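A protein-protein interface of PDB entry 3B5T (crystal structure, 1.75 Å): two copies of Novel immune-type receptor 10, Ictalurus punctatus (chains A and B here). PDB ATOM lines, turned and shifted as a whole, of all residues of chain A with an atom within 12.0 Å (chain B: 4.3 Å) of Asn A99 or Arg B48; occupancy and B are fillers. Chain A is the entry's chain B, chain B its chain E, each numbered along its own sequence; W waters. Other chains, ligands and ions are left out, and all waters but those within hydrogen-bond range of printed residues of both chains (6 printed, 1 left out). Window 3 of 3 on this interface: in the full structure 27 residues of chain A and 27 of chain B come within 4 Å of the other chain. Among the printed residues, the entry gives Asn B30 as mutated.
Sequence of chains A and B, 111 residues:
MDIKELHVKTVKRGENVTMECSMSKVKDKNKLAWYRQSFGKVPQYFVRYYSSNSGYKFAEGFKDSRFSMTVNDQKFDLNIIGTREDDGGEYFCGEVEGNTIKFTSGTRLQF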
ATOM      1  N   MET A   1     -11.566   2.047 -24.781  1.00  0.00           N
ATOM      2  CA  MET A   1     -10.130   2.153 -24.383  1.00  0.00           C
ATOM      3  C   MET A   1      -9.594   0.786 -23.968  1.00  0.00           C
ATOM      4  O   MET A   1     -10.300   0.004 -23.318  1.00  0.00           O
ATOM      5  CB  MET A   1      -9.979   3.132 -23.227  1.00  0.00           C
ATOM      6  CG  MET A   1     -10.791   2.727 -22.004  1.00  0.00           C
ATOM      7  SD  MET A   1     -10.275   3.685 -20.393  1.00  0.00           S
ATOM      8  CE  MET A   1     -10.501   5.535 -21.059  1.00  0.00           C
ATOM      9  N   LYS A  27      -1.365  15.548 -21.485  1.00  0.00           N
ATOM     10  CA  LYS A  27      -1.845  16.749 -22.156  1.00  0.00           C
ATOM     11  C   LYS A  27      -1.671  17.954 -21.253  1.00  0.00           C
ATOM     12  O   LYS A  27      -1.129  18.984 -21.672  1.00  0.00           O
ATOM     13  CB  LYS A  27      -3.314  16.602 -22.572  1.00  0.00           C
ATOM     14  CG  LYS A  27      -3.570  15.651 -23.758  1.00  0.00           C
ATOM     15  CD  LYS A  27      -3.240  14.175 -23.466  1.00  0.00           C
ATOM     16  CE  LYS A  27      -4.044  13.590 -22.303  1.00  0.00           C
ATOM     17  NZ  LYS A  27      -3.395  12.358 -21.773  1.00  0.00           N
ATOM     18  N   ASP A  28      -2.117  17.825 -20.005  1.00  0.00           N
ATOM     19  CA  ASP A  28      -2.018  18.916 -19.054  1.00  0.00           C
ATOM     20  C   ASP A  28      -1.393  18.376 -17.763  1.00  0.00           C
ATOM     21  O   ASP A  28      -2.040  17.663 -16.998  1.00  0.00           O
ATOM     22  CB  ASP A  28      -3.405  19.530 -18.824  1.00  0.00           C
ATOM     23  CG  ASP A  28      -3.376  20.770 -17.928  1.00  0.00           C
ATOM     24  OD1 ASP A  28      -2.331  21.070 -17.326  1.00  0.00           O
ATOM     25  OD2 ASP A  28      -4.415  21.441 -17.810  1.00  0.00           O
ATOM     26  N   LYS A  31      -3.044  18.403 -14.287  1.00  0.00           N
ATOM     27  CA  LYS A  31      -4.134  17.460 -14.036  1.00  0.00           C
ATOM     28  C   LYS A  31      -3.660  16.061 -13.700  1.00  0.00           C
ATOM     29  O   LYS A  31      -4.470  15.142 -13.585  1.00  0.00           O
ATOM     30  CB  LYS A  31      -5.068  17.387 -15.257  1.00  0.00           C
ATOM     31  CG  LYS A  31      -5.624  18.720 -15.715  1.00  0.00           C
ATOM     32  CD  LYS A  31      -6.542  19.302 -14.716  1.00  0.00           C
ATOM     33  CE  LYS A  31      -7.163  20.576 -15.245  1.00  0.00           C
ATOM     34  NZ  LYS A  31      -8.165  20.228 -16.262  1.00  0.00           N
ATOM     35  N   TYR A  35      -2.540   8.168  -7.164  1.00  0.00           N
ATOM     36  CA  TYR A  35      -3.613   7.732  -6.267  1.00  0.00           C
ATOM     37  C   TYR A  35      -3.116   6.512  -5.548  1.00  0.00           C
ATOM     38  O   TYR A  35      -2.526   5.622  -6.175  1.00  0.00           O
ATOM     39  CB  TYR A  35      -4.908   7.456  -7.089  1.00  0.00           C
ATOM     40  CG  TYR A  35      -5.400   8.764  -7.655  1.00  0.00           C
ATOM     41  CD1 TYR A  35      -6.402   9.489  -7.018  1.00  0.00           C
ATOM     42  CD2 TYR A  35      -4.819   9.312  -8.794  1.00  0.00           C
ATOM     43  CE1 TYR A  35      -6.821  10.740  -7.500  1.00  0.00           C
ATOM     44  CE2 TYR A  35      -5.223  10.560  -9.295  1.00  0.00           C
ATOM     45  CZ  TYR A  35      -6.230  11.265  -8.650  1.00  0.00           C
ATOM     46  OH  TYR A  35      -6.617  12.503  -9.133  1.00  0.00           O
ATOM     47  N   GLY A  94      -3.017   8.940 -12.852  1.00  0.00           N
ATOM     48  CA  GLY A  94      -4.142   9.383 -13.674  1.00  0.00           C
ATOM     49  C   GLY A  94      -4.121  10.858 -14.001  1.00  0.00           C
ATOM     50  O   GLY A  94      -3.630  11.682 -13.209  1.00  0.00           O
ATOM     51  N   GLU A  95      -4.695  11.185 -15.155  1.00  0.00           N
ATOM     52  CA  GLU A  95      -4.849  12.563 -15.599  1.00  0.00           C
ATOM     53  C   GLU A  95      -6.325  12.910 -15.760  1.00  0.00           C
ATOM     54  O   GLU A  95      -7.065  12.242 -16.513  1.00  0.00           O
ATOM     55  CB  GLU A  95      -4.098  12.789 -16.919  1.00  0.00           C
ATOM     56  CG  GLU A  95      -4.278  14.177 -17.459  1.00  0.00           C
ATOM     57  CD  GLU A  95      -3.554  14.420 -18.801  1.00  0.00           C
ATOM     58  OE1 GLU A  95      -2.861  13.520 -19.308  1.00  0.00           O
ATOM     59  OE2 GLU A  95      -3.690  15.542 -19.329  1.00  0.00           O
ATOM     60  N   VAL A  96      -6.765  13.946 -15.047  1.00  0.00           N
ATOM     61  CA  VAL A  96      -8.119  14.473 -15.231  1.00  0.00           C
ATOM     62  C   VAL A  96      -8.288  15.065 -16.629  1.00  0.00           C
ATOM     63  O   VAL A  96      -7.425  15.806 -17.113  1.00  0.00           O
ATOM     64  CB  VAL A  96      -8.483  15.526 -14.148  1.00  0.00           C
ATOM     65  CG1 VAL A  96      -9.791  16.258 -14.509  1.00  0.00           C
ATOM     66  CG2 VAL A  96      -8.601  14.856 -12.801  1.00  0.00           C
ATOM     67  N   GLU A  97      -9.383  14.686 -17.283  1.00  0.00           N
ATOM     68  CA  GLU A  97      -9.724  15.156 -18.616  1.00  0.00           C
ATOM     69  C   GLU A  97     -11.230  15.440 -18.607  1.00  0.00           C
ATOM     70  O   GLU A  97     -12.041  14.532 -18.812  1.00  0.00           O
ATOM     71  CB  GLU A  97      -9.381  14.080 -19.660  1.00  0.00           C
ATOM     72  CG  GLU A  97      -8.025  13.380 -19.434  1.00  0.00           C
ATOM     73  CD  GLU A  97      -7.650  12.363 -20.497  1.00  0.00           C
ATOM     74  OE1 GLU A  97      -6.458  11.955 -20.509  1.00  0.00           O
ATOM     75  OE2 GLU A  97      -8.520  11.955 -21.299  1.00  0.00           O
ATOM     76  N   GLY A  98     -11.602  16.679 -18.301  1.00  0.00           N
ATOM     77  CA  GLY A  98     -13.017  17.075 -18.258  1.00  0.00           C
ATOM     78  C   GLY A  98     -13.805  16.448 -17.114  1.00  0.00           C
ATOM     79  O   GLY A  98     -13.528  16.708 -15.945  1.00  0.00           O
ATOM     80  N   ASN A  99     -14.793  15.622 -17.463  1.00  0.00           N
ATOM     81  CA  ASN A  99     -15.707  15.028 -16.474  1.00  0.00           C
ATOM     82  C   ASN A  99     -15.153  13.787 -15.787  1.00  0.00           C
ATOM     83  O   ASN A  99     -15.710  13.339 -14.778  1.00  0.00           O
ATOM     84  CB  ASN A  99     -17.031  14.635 -17.135  1.00  0.00           C
ATOM     85  CG  ASN A  99     -17.815  15.829 -17.658  1.00  0.00           C
ATOM     86  OD1 ASN A  99     -18.525  15.714 -18.662  1.00  0.00           O
ATOM     87  ND2 ASN A  99     -17.706  16.966 -16.984  1.00  0.00           N
ATOM     88  N   THR A 100     -14.082  13.228 -16.340  1.00  0.00           N
ATOM     89  CA  THR A 100     -13.556  11.950 -15.856  1.00  0.00           C
ATOM     90  C   THR A 100     -12.042  11.992 -15.721  1.00  0.00           C
ATOM     91  O   THR A 100     -11.386  12.882 -16.264  1.00  0.00           O
ATOM     92  CB  THR A 100     -13.908  10.782 -16.822  1.00  0.00           C
ATOM     93  OG1 THR A 100     -13.381  11.061 -18.121  1.00  0.00           O
ATOM     94  CG2 THR A 100     -15.423  10.584 -16.922  1.00  0.00           C
ATOM     95  N   ILE A 101     -11.502  11.004 -15.030  1.00  0.00           N
ATOM     96  CA  ILE A 101     -10.062  10.811 -14.975  1.00  0.00           C
ATOM     97  C   ILE A 101      -9.659   9.642 -15.871  1.00  0.00           C
ATOM     98  O   ILE A 101     -10.392   8.647 -16.018  1.00  0.00           O
ATOM     99  CB  ILE A 101      -9.572  10.577 -13.531  1.00  0.00           C
ATOM    100  CG1 ILE A 101      -8.039  10.618 -13.463  1.00  0.00           C
ATOM    101  CG2 ILE A 101     -10.237   9.312 -12.885  1.00  0.00           C
ATOM    102  CD1 ILE A 101      -7.478  10.777 -12.018  1.00  0.00           C
ATOM    103  N   LYS A 102      -8.506   9.752 -16.503  1.00  0.00           N
ATOM    104  CA  LYS A 102      -8.011   8.572 -17.147  1.00  0.00           C
ATOM    105  C   LYS A 102      -6.687   8.099 -16.562  1.00  0.00           C
ATOM    106  O   LYS A 102      -5.719   8.863 -16.477  1.00  0.00           O
ATOM    107  CB  LYS A 102      -8.040   8.727 -18.653  1.00  0.00           C
ATOM    108  CG  LYS A 102      -6.860   9.235 -19.254  1.00  0.00           C
ATOM    109  CD  LYS A 102      -6.263   8.184 -20.144  1.00  0.00           C
ATOM    110  CE  LYS A 102      -5.345   8.854 -21.141  1.00  0.00           C
ATOM    111  NZ  LYS A 102      -4.614   9.997 -20.515  1.00  0.00           N
ATOM    112  N   PHE A 103      -6.671   6.839 -16.143  1.00  0.00           N
ATOM    113  CA  PHE A 103      -5.508   6.269 -15.507  1.00  0.00           C
ATOM    114  C   PHE A 103      -4.646   5.647 -16.568  1.00  0.00           C
ATOM    115  O   PHE A 103      -5.133   4.878 -17.404  1.00  0.00           O
ATOM    116  CB  PHE A 103      -5.912   5.224 -14.469  1.00  0.00           C
ATOM    117  CG  PHE A 103      -6.628   5.797 -13.296  1.00  0.00           C
ATOM    118  CD1 PHE A 103      -5.919   6.481 -12.309  1.00  0.00           C
ATOM    119  CD2 PHE A 103      -8.006   5.663 -13.169  1.00  0.00           C
ATOM    120  CE1 PHE A 103      -6.583   7.026 -11.212  1.00  0.00           C
ATOM    121  CE2 PHE A 103      -8.681   6.189 -12.078  1.00  0.00           C
ATOM    122  CZ  PHE A 103      -7.960   6.881 -11.082  1.00  0.00           C
ATOM    123  N   ASN B  30     -22.162  16.484 -13.249  1.00  0.00           N
ATOM    124  CA  ASN B  30     -21.569  16.181 -14.552  1.00  0.00           C
ATOM    125  C   ASN B  30     -20.186  15.537 -14.430  1.00  0.00           C
ATOM    126  O   ASN B  30     -19.718  14.885 -15.363  1.00  0.00           O
ATOM    127  CB  ASN B  30     -21.468  17.431 -15.408  1.00  0.00           C
ATOM    128  CG  ASN B  30     -22.825  17.982 -15.791  1.00  0.00           C
ATOM    129  OD1 ASN B  30     -23.673  17.268 -16.335  1.00  0.00           O
ATOM    130  ND2 ASN B  30     -23.038  19.258 -15.507  1.00  0.00           N
ATOM    131  N   LYS B  31     -19.545  15.719 -13.281  1.00  0.00           N
ATOM    132  CA  LYS B  31     -18.191  15.211 -13.075  1.00  0.00           C
ATOM    133  C   LYS B  31     -18.184  13.946 -12.221  1.00  0.00           C
ATOM    134  O   LYS B  31     -17.145  13.549 -11.676  1.00  0.00           O
ATOM    135  CB  LYS B  31     -17.335  16.293 -12.427  1.00  0.00           C
ATOM    136  CG  LYS B  31     -17.161  17.488 -13.334  1.00  0.00           C
ATOM    137  CD  LYS B  31     -16.190  18.478 -12.761  1.00  0.00           C
ATOM    138  CE  LYS B  31     -15.918  19.555 -13.786  1.00  0.00           C
ATOM    139  NZ  LYS B  31     -17.121  20.418 -13.893  1.00  0.00           N
ATOM    140  N   LEU B  32     -19.359  13.334 -12.089  1.00  0.00           N
ATOM    141  CA  LEU B  32     -19.518  12.149 -11.271  1.00  0.00           C
ATOM    142  C   LEU B  32     -19.551  10.886 -12.150  1.00  0.00           C
ATOM    143  O   LEU B  32     -20.273  10.840 -13.141  1.00  0.00           O
ATOM    144  CB  LEU B  32     -20.816  12.245 -10.460  1.00  0.00           C
ATOM    145  CG  LEU B  32     -21.098  11.149  -9.434  1.00  0.00           C
ATOM    146  CD1 LEU B  32     -20.148  11.200  -8.241  1.00  0.00           C
ATOM    147  CD2 LEU B  32     -22.550  11.316  -8.966  1.00  0.00           C
ATOM    148  N   ALA B  33     -18.760   9.884 -11.773  1.00  0.00           N
ATOM    149  CA  ALA B  33     -18.686   8.635 -12.550  1.00  0.00           C
ATOM    150  C   ALA B  33     -18.272   7.460 -11.687  1.00  0.00           C
ATOM    151  O   ALA B  33     -17.660   7.628 -10.599  1.00  0.00           O
ATOM    152  CB  ALA B  33     -17.705   8.792 -13.730  1.00  0.00           C
ATOM    153  N   TYR B  45     -12.647   4.249 -16.653  1.00  0.00           N
ATOM    154  CA  TYR B  45     -13.942   4.923 -16.633  1.00  0.00           C
ATOM    155  C   TYR B  45     -15.055   3.983 -17.160  1.00  0.00           C
ATOM    156  O   TYR B  45     -14.912   3.366 -18.228  1.00  0.00           O
ATOM    157  CB  TYR B  45     -13.835   6.218 -17.453  1.00  0.00           C
ATOM    158  CG  TYR B  45     -15.102   6.717 -18.079  1.00  0.00           C
ATOM    159  CD1 TYR B  45     -16.250   6.944 -17.311  1.00  0.00           C
ATOM    160  CD2 TYR B  45     -15.141   7.023 -19.429  1.00  0.00           C
ATOM    161  CE1 TYR B  45     -17.420   7.413 -17.900  1.00  0.00           C
ATOM    162  CE2 TYR B  45     -16.304   7.520 -20.026  1.00  0.00           C
ATOM    163  CZ  TYR B  45     -17.434   7.695 -19.255  1.00  0.00           C
ATOM    164  OH  TYR B  45     -18.583   8.170 -19.858  1.00  0.00           O
ATOM    165  N   VAL B  47     -18.942   4.440 -16.298  1.00  0.00           N
ATOM    166  CA  VAL B  47     -20.211   5.120 -16.599  1.00  0.00           C
ATOM    167  C   VAL B  47     -20.254   6.455 -15.876  1.00  0.00           C
ATOM    168  O   VAL B  47     -19.826   6.555 -14.726  1.00  0.00           O
ATOM    169  CB  VAL B  47     -21.437   4.262 -16.196  1.00  0.00           C
ATOM    170  CG1 VAL B  47     -21.326   3.780 -14.740  1.00  0.00           C
ATOM    171  CG2 VAL B  47     -22.766   5.015 -16.441  1.00  0.00           C
ATOM    172  N   ARG B  48     -20.775   7.464 -16.559  1.00  0.00           N
ATOM    173  CA  ARG B  48     -20.866   8.798 -15.978  1.00  0.00           C
ATOM    174  C   ARG B  48     -22.315   9.277 -15.856  1.00  0.00           C
ATOM    175  O   ARG B  48     -23.200   8.818 -16.586  1.00  0.00           O
ATOM    176  CB  ARG B  48     -20.026   9.782 -16.810  1.00  0.00           C
ATOM    177  CG  ARG B  48     -20.555  10.081 -18.219  1.00  0.00           C
ATOM    178  CD  ARG B  48     -19.565  10.973 -18.926  1.00  0.00           C
ATOM    179  NE  ARG B  48     -19.805  11.121 -20.363  1.00  0.00           N
ATOM    180  CZ  ARG B  48     -20.400  12.164 -20.933  1.00  0.00           C
ATOM    181  NH1 ARG B  48     -20.860  13.168 -20.194  1.00  0.00           N
ATOM    182  NH2 ARG B  48     -20.535  12.199 -22.258  1.00  0.00           N
ATOM    183  N   TYR B  49     -22.541  10.189 -14.909  1.00  0.00           N
ATOM    184  CA  TYR B  49     -23.812  10.900 -14.824  1.00  0.00           C
ATOM    185  C   TYR B  49     -24.069  11.599 -16.164  1.00  0.00           C
ATOM    186  O   TYR B  49     -23.140  12.044 -16.829  1.00  0.00           O
ATOM    187  CB  TYR B  49     -23.792  11.899 -13.672  1.00  0.00           C
ATOM    188  CG  TYR B  49     -25.026  12.777 -13.651  1.00  0.00           C
ATOM    189  CD1 TYR B  49     -26.171  12.356 -12.996  1.00  0.00           C
ATOM    190  CD2 TYR B  49     -25.049  14.003 -14.319  1.00  0.00           C
ATOM    191  CE1 TYR B  49     -27.330  13.143 -12.977  1.00  0.00           C
ATOM    192  CE2 TYR B  49     -26.199  14.796 -14.321  1.00  0.00           C
ATOM    193  CZ  TYR B  49     -27.330  14.354 -13.640  1.00  0.00           C
ATOM    194  OH  TYR B  49     -28.482  15.118 -13.619  1.00  0.00           O
ATOM    195  N   TYR B  50     -25.329  11.666 -16.586  1.00  0.00           N
ATOM    196  CA  TYR B  50     -25.656  12.332 -17.834  1.00  0.00           C
ATOM    197  C   TYR B  50     -27.063  12.939 -17.738  1.00  0.00           C
ATOM    198  O   TYR B  50     -27.995  12.283 -17.279  1.00  0.00           O
ATOM    199  CB  TYR B  50     -25.543  11.339 -18.995  1.00  0.00           C
ATOM    200  CG  TYR B  50     -25.567  11.975 -20.358  1.00  0.00           C
ATOM    201  CD1 TYR B  50     -24.484  12.727 -20.815  1.00  0.00           C
ATOM    202  CD2 TYR B  50     -26.668  11.810 -21.203  1.00  0.00           C
ATOM    203  CE1 TYR B  50     -24.500  13.311 -22.072  1.00  0.00           C
ATOM    204  CE2 TYR B  50     -26.698  12.393 -22.465  1.00  0.00           C
ATOM    205  CZ  TYR B  50     -25.612  13.142 -22.892  1.00  0.00           C
ATOM    206  OH  TYR B  50     -25.632  13.728 -24.145  1.00  0.00           O
ATOM    207  N   TYR B  56     -27.666   8.667 -17.034  1.00  0.00           N
ATOM    208  CA  TYR B  56     -26.310   8.124 -17.108  1.00  0.00           C
ATOM    209  C   TYR B  56     -25.919   7.747 -18.520  1.00  0.00           C
ATOM    210  O   TYR B  56     -26.781   7.561 -19.382  1.00  0.00           O
ATOM    211  CB  TYR B  56     -26.160   6.919 -16.188  1.00  0.00           C
ATOM    212  CG  TYR B  56     -27.077   5.755 -16.512  1.00  0.00           C
ATOM    213  CD1 TYR B  56     -26.704   4.773 -17.441  1.00  0.00           C
ATOM    214  CD2 TYR B  56     -28.312   5.627 -15.873  1.00  0.00           C
ATOM    215  CE1 TYR B  56     -27.553   3.703 -17.726  1.00  0.00           C
ATOM    216  CE2 TYR B  56     -29.149   4.566 -16.152  1.00  0.00           C
ATOM    217  CZ  TYR B  56     -28.765   3.615 -17.074  1.00  0.00           C
ATOM    218  OH  TYR B  56     -29.618   2.563 -17.326  1.00  0.00           O
ATOM    219  N   LYS B  57     -24.613   7.620 -18.750  1.00  0.00           N
ATOM    220  CA  LYS B  57     -24.116   7.143 -20.024  1.00  0.00           C
ATOM    221  C   LYS B  57     -22.901   6.281 -19.796  1.00  0.00           C
ATOM    222  O   LYS B  57     -21.895   6.762 -19.280  1.00  0.00           O
ATOM    223  CB  LYS B  57     -23.740   8.321 -20.928  1.00  0.00           C
ATOM    224  CG  LYS B  57     -22.993   7.941 -22.199  1.00  0.00           C
ATOM    225  CD  LYS B  57     -23.915   7.709 -23.407  1.00  0.00           C
ATOM    226  CE  LYS B  57     -24.648   8.978 -23.880  1.00  0.00           C
ATOM    227  NZ  LYS B  57     -23.912  10.241 -23.567  1.00  0.00           N
ATOM    228  N   PHE B  76     -26.796   7.390  -6.858  1.00  0.00           N
ATOM    229  CA  PHE B  76     -26.019   7.216  -8.079  1.00  0.00           C
ATOM    230  C   PHE B  76     -25.523   5.757  -8.083  1.00  0.00           C
ATOM    231  O   PHE B  76     -24.315   5.469  -8.044  1.00  0.00           O
ATOM    232  CB  PHE B  76     -24.871   8.231  -8.171  1.00  0.00           C
ATOM    233  CG  PHE B  76     -24.181   8.242  -9.514  1.00  0.00           C
ATOM    234  CD1 PHE B  76     -24.875   8.574 -10.678  1.00  0.00           C
ATOM    235  CD2 PHE B  76     -22.825   7.914  -9.608  1.00  0.00           C
ATOM    236  CE1 PHE B  76     -24.239   8.583 -11.923  1.00  0.00           C
ATOM    237  CE2 PHE B  76     -22.172   7.921 -10.851  1.00  0.00           C
ATOM    238  CZ  PHE B  76     -22.869   8.253 -12.000  1.00  0.00           C
ATOM    239  N   VAL B  96     -14.745  14.339 -10.160  1.00  0.00           N
ATOM    240  CA  VAL B  96     -13.606  15.196 -10.543  1.00  0.00           C
ATOM    241  C   VAL B  96     -13.789  16.586  -9.934  1.00  0.00           C
ATOM    242  O   VAL B  96     -14.853  17.190 -10.073  1.00  0.00           O
ATOM    243  CB  VAL B  96     -13.445  15.293 -12.065  1.00  0.00           C
ATOM    244  CG1 VAL B  96     -12.476  16.402 -12.439  1.00  0.00           C
ATOM    245  CG2 VAL B  96     -12.932  13.979 -12.619  1.00  0.00           C
HETATM  246  O   HOH W   1      -9.842   6.031 -15.878  1.00  0.00           O
HETATM  247  O   HOH W   2     -15.503  11.389 -12.633  1.00  0.00           O
HETATM  248  O   HOH W   3     -17.370  13.384 -20.652  1.00  0.00           O
HETATM  249  O   HOH W   4     -10.395   5.249 -18.175  1.00  0.00           O
HETATM  250  O   HOH W   5     -18.989  19.768 -15.885  1.00  0.00           O
HETATM  251  O   HOH W   6     -13.518   3.650 -20.497  1.00  0.00           O
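The backbone carbonyl oxygen of Lys B31 lies close to the backbone carbonyl oxygen of Asn A99, 3.4 Å away. ND2 of Asn A99 sits close to O of Asn B30 (3.3 Å).
The side-chain hydroxyl (OH) of Tyr B45 sits close to the guanidinium group (NE) of Arg B48 (3.2 Å). N of Lys B57 sits at hydrogen-bond distance from O of Arg B48 (2.8 Å). The backbone NH (N) of Val A96 is in hydrogen-bond range of the backbone carbonyl oxygen (O) of Lys A31 (3.0 Å). The backbone NH (N) of Val B96 is in hydrogen-bond range of the backbone carbonyl oxygen (O) of Lys B31 (2.9 Å).
Val A96 touches Val B96. Gly A98 touches Val B96 (O to CG1, 3.7 Å). NH1 of Arg B48 touches OD1 of Asn A99, at 3.8 Å. Val B96 touches Asn A99. Thr A100 touches Tyr B45. Val B96 touches Thr A100.
Asn A99 touches just these residues of chain B: Asn B30 (3.1 Å), Lys B31 (3.4 Å), Arg B48 (3.8 Å) and Val B96 (3.6 Å). Of the printed residues of chain A, Arg B48 touches Asn A99 (3.8 Å). Asn B30 touches just one residue of chain A: Asn A99. No residue of chain A comes within 4 Å of Ala B33. No residue of chain A comes within 4 Å of Tyr B50. No residue of chain A comes within 4 Å of Lys B57. Of chain A, only Val A96 (3.4 Å), Gly A98 (3.7 Å), Asn A99 (3.6 Å) and Thr A100 (3.8 Å) come within 4 Å of Val B96. Of the printed residues of chain B, Gly A98 touches Val B96. Of the printed residues of chain B, Thr A100 touches Tyr B45 (3.8 Å) and Val B96 (3.8 Å). The nearest residue of chain A that does not touch Arg B48 is Thr A100 (4.6 Å).
Hydrophobic or aromatic side chains of chain B that line the printed part of chain A: Tyr B45 and Val B96. Of the 15 printed residues of chain A, 4 touch a printed residue of chain B. Printed residues of chain A that touch a printed residue of chain B: Val A96, Gly A98, Asn A99 and Thr A100. Hydrophobic or aromatic side chains of chain A within 4 Å of the printed part of chain B: Val A96. Among the printed residues, no Asp or Glu carboxylate lies within 4 Å of a Lys or Arg side-chain nitrogen of the other chain.
Val A96 touches its own counterpart, Val B96. Of the 8 pairs that touch across the chains among the printed residues, 1 has its exchanged pair printed and touching as well.
Water W1 lies within hydrogen-bond range of the backbone carbonyl oxygen (O) of Ile A101, the backbone NH (N) of Phe A103 and the backbone NH (N) of Tyr B45. Water W6 lies within hydrogen-bond range of O of Tyr B45 (2.7 Å) and SD of Met A1 (3.2 Å). Water W4 bridges SD of Met A1 (2.7 Å) and N of Tyr B45 (2.9 Å). Water W5 lies within hydrogen-bond range of NZ of Lys B31 (2.8 Å) and ND2 of Asn A99 (3.3 Å). Water W2 lies within hydrogen-bond range of the backbone carbonyl oxygen of Lys B31 and the backbone carbonyl oxygen of Asn A99. Water W3 lies within hydrogen-bond range of the side-chain amide oxygen of Asn A99 (3.3 Å) and the guanidinium group of Arg B48 (3.3 Å).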
